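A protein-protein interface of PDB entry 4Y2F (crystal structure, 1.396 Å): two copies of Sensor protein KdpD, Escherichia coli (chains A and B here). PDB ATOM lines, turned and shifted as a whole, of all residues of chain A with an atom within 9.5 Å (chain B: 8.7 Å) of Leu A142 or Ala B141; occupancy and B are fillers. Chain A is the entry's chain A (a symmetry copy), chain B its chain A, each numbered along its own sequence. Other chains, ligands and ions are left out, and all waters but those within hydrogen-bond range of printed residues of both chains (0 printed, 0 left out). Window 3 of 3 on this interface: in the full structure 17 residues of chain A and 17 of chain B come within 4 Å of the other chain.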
ATOM      1  N   ARG A 134     -13.318  -9.861  17.466  1.00  0.00           N
ATOM      2  CA  ARG A 134     -14.574 -10.199  16.816  1.00  0.00           C
ATOM      3  C   ARG A 134     -14.362 -10.535  15.344  1.00  0.00           C
ATOM      4  O   ARG A 134     -14.862 -11.552  14.851  1.00  0.00           O
ATOM      5  CB  ARG A 134     -15.571  -9.056  16.982  1.00  0.00           C
ATOM      6  CG  ARG A 134     -16.896  -9.345  16.314  1.00  0.00           C
ATOM      7  CD  ARG A 134     -17.888  -8.233  16.565  1.00  0.00           C
ATOM      8  NE  ARG A 134     -17.475  -6.985  15.929  1.00  0.00           N
ATOM      9  CZ  ARG A 134     -17.056  -5.908  16.586  1.00  0.00           C
ATOM     10  NH1 ARG A 134     -16.985  -5.916  17.915  1.00  0.00           N
ATOM     11  NH2 ARG A 134     -16.705  -4.820  15.911  1.00  0.00           N
ATOM     12  N   LEU A 135     -13.619  -9.690  14.624  1.00  0.00           N
ATOM     13  CA  LEU A 135     -13.425  -9.933  13.196  1.00  0.00           C
ATOM     14  C   LEU A 135     -12.610 -11.197  12.945  1.00  0.00           C
ATOM     15  O   LEU A 135     -12.931 -11.981  12.045  1.00  0.00           O
ATOM     16  CB  LEU A 135     -12.753  -8.732  12.534  1.00  0.00           C
ATOM     17  CG  LEU A 135     -13.568  -7.449  12.398  1.00  0.00           C
ATOM     18  CD1 LEU A 135     -12.758  -6.427  11.633  1.00  0.00           C
ATOM     19  CD2 LEU A 135     -14.891  -7.709  11.703  1.00  0.00           C
ATOM     20  N   THR A 136     -11.544 -11.399  13.724  1.00  0.00           N
ATOM     21  CA  THR A 136     -10.693 -12.572  13.544  1.00  0.00           C
ATOM     22  C   THR A 136     -11.474 -13.857  13.783  1.00  0.00           C
ATOM     23  O   THR A 136     -11.430 -14.791  12.972  1.00  0.00           O
ATOM     24  CB  THR A 136      -9.501 -12.481  14.501  1.00  0.00           C
ATOM     25  OG1 THR A 136      -8.663 -11.387  14.114  1.00  0.00           O
ATOM     26  CG2 THR A 136      -8.692 -13.781  14.474  1.00  0.00           C
ATOM     27  N   LYS A 137     -12.195 -13.926  14.901  1.00  0.00           N
ATOM     28  CA  LYS A 137     -12.912 -15.153  15.224  1.00  0.00           C
ATOM     29  C   LYS A 137     -14.066 -15.407  14.261  1.00  0.00           C
ATOM     30  O   LYS A 137     -14.366 -16.566  13.949  1.00  0.00           O
ATOM     31  CB  LYS A 137     -13.356 -15.140  16.688  1.00  0.00           C
ATOM     32  CG  LYS A 137     -12.181 -15.177  17.664  1.00  0.00           C
ATOM     33  CD  LYS A 137     -12.629 -15.338  19.109  1.00  0.00           C
ATOM     34  CE  LYS A 137     -11.444 -15.669  20.015  1.00  0.00           C
ATOM     35  NZ  LYS A 137     -11.792 -15.612  21.464  1.00  0.00           N
ATOM     36  N   LEU A 138     -14.709 -14.348  13.760  1.00  0.00           N
ATOM     37  CA  LEU A 138     -15.793 -14.533  12.799  1.00  0.00           C
ATOM     38  C   LEU A 138     -15.265 -15.025  11.458  1.00  0.00           C
ATOM     39  O   LEU A 138     -15.815 -15.968  10.874  1.00  0.00           O
ATOM     40  CB  LEU A 138     -16.586 -13.237  12.637  1.00  0.00           C
ATOM     41  CG  LEU A 138     -17.672 -13.039  13.695  1.00  0.00           C
ATOM     42  CD1 LEU A 138     -18.231 -11.615  13.655  1.00  0.00           C
ATOM     43  CD2 LEU A 138     -18.781 -14.064  13.505  1.00  0.00           C
ATOM     44  N   ALA A 139     -14.198 -14.397  10.953  1.00  0.00           N
ATOM     45  CA  ALA A 139     -13.587 -14.860   9.709  1.00  0.00           C
ATOM     46  C   ALA A 139     -13.183 -16.325   9.808  1.00  0.00           C
ATOM     47  O   ALA A 139     -13.361 -17.091   8.853  1.00  0.00           O
ATOM     48  CB  ALA A 139     -12.381 -13.986   9.361  1.00  0.00           C
ATOM     49  N   ALA A 140     -12.646 -16.737  10.958  1.00  0.00           N
ATOM     50  CA  ALA A 140     -12.284 -18.140  11.137  1.00  0.00           C
ATOM     51  C   ALA A 140     -13.520 -19.028  11.148  1.00  0.00           C
ATOM     52  O   ALA A 140     -13.513 -20.119  10.563  1.00  0.00           O
ATOM     53  CB  ALA A 140     -11.481 -18.318  12.426  1.00  0.00           C
ATOM     54  N   ALA A 141     -14.591 -18.575  11.806  1.00  0.00           N
ATOM     55  CA  ALA A 141     -15.837 -19.332  11.830  1.00  0.00           C
ATOM     56  C   ALA A 141     -16.367 -19.587  10.426  1.00  0.00           C
ATOM     57  O   ALA A 141     -16.979 -20.632  10.173  1.00  0.00           O
ATOM     58  CB  ALA A 141     -16.880 -18.581  12.656  1.00  0.00           C
ATOM     59  N   LEU A 142     -16.124 -18.662   9.496  1.00  0.00           N
ATOM     60  CA  LEU A 142     -16.709 -18.725   8.164  1.00  0.00           C
ATOM     61  C   LEU A 142     -15.736 -19.142   7.070  1.00  0.00           C
ATOM     62  O   LEU A 142     -16.187 -19.566   6.002  1.00  0.00           O
ATOM     63  CB  LEU A 142     -17.323 -17.367   7.795  1.00  0.00           C
ATOM     64  CG  LEU A 142     -18.377 -16.849   8.777  1.00  0.00           C
ATOM     65  CD1 LEU A 142     -18.726 -15.399   8.486  1.00  0.00           C
ATOM     66  CD2 LEU A 142     -19.626 -17.723   8.732  1.00  0.00           C
ATOM     67  N   GLU A 143     -14.431 -19.040   7.301  1.00  0.00           N
ATOM     68  CA  GLU A 143     -13.448 -19.342   6.264  1.00  0.00           C
ATOM     69  C   GLU A 143     -12.396 -20.342   6.736  1.00  0.00           C
ATOM     70  O   GLU A 143     -11.869 -21.124   5.942  1.00  0.00           O
ATOM     71  CB  GLU A 143     -12.782 -18.059   5.780  1.00  0.00           C
ATOM     72  N   ARG B 134     -19.999 -10.650  20.481  1.00  0.00           N
ATOM     73  CA  ARG B 134     -19.092 -11.679  19.998  1.00  0.00           C
ATOM     74  C   ARG B 134     -19.743 -13.057  20.050  1.00  0.00           C
ATOM     75  O   ARG B 134     -19.696 -13.814  19.074  1.00  0.00           O
ATOM     76  CB  ARG B 134     -17.795 -11.652  20.802  1.00  0.00           C
ATOM     77  CG  ARG B 134     -16.815 -12.712  20.353  1.00  0.00           C
ATOM     78  CD  ARG B 134     -15.512 -12.606  21.111  1.00  0.00           C
ATOM     79  NE  ARG B 134     -15.684 -12.910  22.529  1.00  0.00           N
ATOM     80  CZ  ARG B 134     -15.598 -12.013  23.507  1.00  0.00           C
ATOM     81  NH1 ARG B 134     -15.345 -10.737  23.228  1.00  0.00           N
ATOM     82  NH2 ARG B 134     -15.769 -12.395  24.766  1.00  0.00           N
ATOM     83  N   LEU B 135     -20.357 -13.402  21.185  1.00  0.00           N
ATOM     84  CA  LEU B 135     -20.954 -14.731  21.312  1.00  0.00           C
ATOM     85  C   LEU B 135     -22.138 -14.909  20.368  1.00  0.00           C
ATOM     86  O   LEU B 135     -22.287 -15.965  19.744  1.00  0.00           O
ATOM     87  CB  LEU B 135     -21.385 -14.990  22.753  1.00  0.00           C
ATOM     88  CG  LEU B 135     -20.289 -15.175  23.800  1.00  0.00           C
ATOM     89  CD1 LEU B 135     -20.924 -15.517  25.127  1.00  0.00           C
ATOM     90  CD2 LEU B 135     -19.309 -16.255  23.384  1.00  0.00           C
ATOM     91  N   THR B 136     -22.995 -13.890  20.265  1.00  0.00           N
ATOM     92  CA  THR B 136     -24.168 -13.977  19.401  1.00  0.00           C
ATOM     93  C   THR B 136     -23.762 -14.162  17.945  1.00  0.00           C
ATOM     94  O   THR B 136     -24.272 -15.049  17.248  1.00  0.00           O
ATOM     95  CB  THR B 136     -25.013 -12.712  19.568  1.00  0.00           C
ATOM     96  OG1 THR B 136     -25.562 -12.678  20.889  1.00  0.00           O
ATOM     97  CG2 THR B 136     -26.147 -12.685  18.540  1.00  0.00           C
ATOM     98  N   LYS B 137     -22.845 -13.325  17.463  1.00  0.00           N
ATOM     99  CA  LYS B 137     -22.462 -13.402  16.059  1.00  0.00           C
ATOM    100  C   LYS B 137     -21.701 -14.686  15.748  1.00  0.00           C
ATOM    101  O   LYS B 137     -21.838 -15.233  14.647  1.00  0.00           O
ATOM    102  CB  LYS B 137     -21.693 -12.146  15.647  1.00  0.00           C
ATOM    103  CG  LYS B 137     -22.555 -10.884  15.685  1.00  0.00           C
ATOM    104  CD  LYS B 137     -21.838  -9.672  15.112  1.00  0.00           C
ATOM    105  CE  LYS B 137     -22.812  -8.516  14.889  1.00  0.00           C
ATOM    106  NZ  LYS B 137     -22.123  -7.239  14.546  1.00  0.00           N
ATOM    107  N   LEU B 138     -20.918 -15.198  16.703  1.00  0.00           N
ATOM    108  CA  LEU B 138     -20.202 -16.449  16.474  1.00  0.00           C
ATOM    109  C   LEU B 138     -21.158 -17.634  16.426  1.00  0.00           C
ATOM    110  O   LEU B 138     -21.066 -18.481  15.528  1.00  0.00           O
ATOM    111  CB  LEU B 138     -19.129 -16.650  17.542  1.00  0.00           C
ATOM    112  CG  LEU B 138     -17.810 -15.939  17.238  1.00  0.00           C
ATOM    113  CD1 LEU B 138     -16.887 -15.938  18.458  1.00  0.00           C
ATOM    114  CD2 LEU B 138     -17.129 -16.588  16.041  1.00  0.00           C
ATOM    115  N   ALA B 139     -22.084 -17.711  17.388  1.00  0.00           N
ATOM    116  CA  ALA B 139     -23.085 -18.774  17.367  1.00  0.00           C
ATOM    117  C   ALA B 139     -23.864 -18.771  16.058  1.00  0.00           C
ATOM    118  O   ALA B 139     -24.154 -19.834  15.497  1.00  0.00           O
ATOM    119  CB  ALA B 139     -24.030 -18.628  18.560  1.00  0.00           C
ATOM    120  N   ALA B 140     -24.203 -17.584  15.549  1.00  0.00           N
ATOM    121  CA  ALA B 140     -24.904 -17.508  14.270  1.00  0.00           C
ATOM    122  C   ALA B 140     -24.017 -17.985  13.129  1.00  0.00           C
ATOM    123  O   ALA B 140     -24.483 -18.691  12.226  1.00  0.00           O
ATOM    124  CB  ALA B 140     -25.387 -16.080  14.017  1.00  0.00           C
ATOM    125  N   ALA B 141     -22.735 -17.611  13.156  1.00  0.00           N
ATOM    126  CA  ALA B 141     -21.797 -18.060  12.134  1.00  0.00           C
ATOM    127  C   ALA B 141     -21.720 -19.579  12.068  1.00  0.00           C
ATOM    128  O   ALA B 141     -21.520 -20.145  10.986  1.00  0.00           O
ATOM    129  CB  ALA B 141     -20.412 -17.477  12.413  1.00  0.00           C
ATOM    130  N   LEU B 142     -21.900 -20.256  13.203  1.00  0.00           N
ATOM    131  CA  LEU B 142     -21.699 -21.695  13.290  1.00  0.00           C
ATOM    132  C   LEU B 142     -22.985 -22.505  13.368  1.00  0.00           C
ATOM    133  O   LEU B 142     -22.950 -23.707  13.089  1.00  0.00           O
ATOM    134  CB  LEU B 142     -20.823 -22.032  14.506  1.00  0.00           C
ATOM    135  CG  LEU B 142     -19.459 -21.337  14.529  1.00  0.00           C
ATOM    136  CD1 LEU B 142     -18.784 -21.508  15.879  1.00  0.00           C
ATOM    137  CD2 LEU B 142     -18.570 -21.868  13.410  1.00  0.00           C
ATOM    138  N   GLU B 143     -24.108 -21.891  13.730  1.00  0.00           N
ATOM    139  CA  GLU B 143     -25.357 -22.628  13.907  1.00  0.00           C
ATOM    140  C   GLU B 143     -26.507 -22.016  13.114  1.00  0.00           C
ATOM    141  O   GLU B 143     -27.416 -22.724  12.674  1.00  0.00           O
ATOM    142  CB  GLU B 143     -25.715 -22.709  15.387  1.00  0.00           C
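Lys A137 touches Leu B138 (O to CD2, 3.5 Å).
O of Lys B137 touches CD2 of Leu A138, at 3.5 Å.
CD2 of Leu B138 touches CD2 of Leu A138, at 3.9 Å.
Leu A138 touches Ala B141.
Ala A141 touches Leu B138.
CB of Ala B141 touches CB of Ala A141, 3.7 Å away.
CB of Ala A141 touches CD2 of Leu B142, at 3.8 Å.
Leu A142 touches Ala B141 (CD2 to CB, 3.8 Å).
Of the printed residues of chain B, Lys A137 touches Leu B138 (3.5 Å).
Leu A142 touches one residue of chain B.
Printed residues of chain A within 4 Å of Lys B137: Leu A138.
Printed residues of chain A within 4 Å of Leu B138: Lys A137 (3.5 Å), Leu A138 (3.9 Å) and Ala A141 (3.9 Å).
The nearest residue of chain B that does not touch Leu A142 is Leu B142 (5.6 Å).
The nearest printed residue of chain B that does not touch Leu A138 is Arg B134 (5.6 Å).
Of the 10 printed residues of chain A, 4 touch a printed residue of chain B.
Of the 10 printed residues of chain B, 4 touch a printed residue of chain A.
Hydrophobic or aromatic side chains of chain B that line the printed part of chain A: Leu B138, Ala B141 and Leu B142.
Along chain B the printed residues that touch a printed residue of chain A span positions 137 to 142.
Lys A137 touches Leu B138, and with the chains exchanged Leu A138 touches Lys B137.
Leu B138 touches its own counterpart, Leu A138.
Leu A138 touches Ala B141, and with the chains exchanged Ala A141 touches Leu B138.
Ala A141 touches Leu B142, and with the chains exchanged Leu A142 touches Ala B141.
Of the 8 pairs that touch across the chains among the printed residues, 8 have their exchanged pair printed and touching as well.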
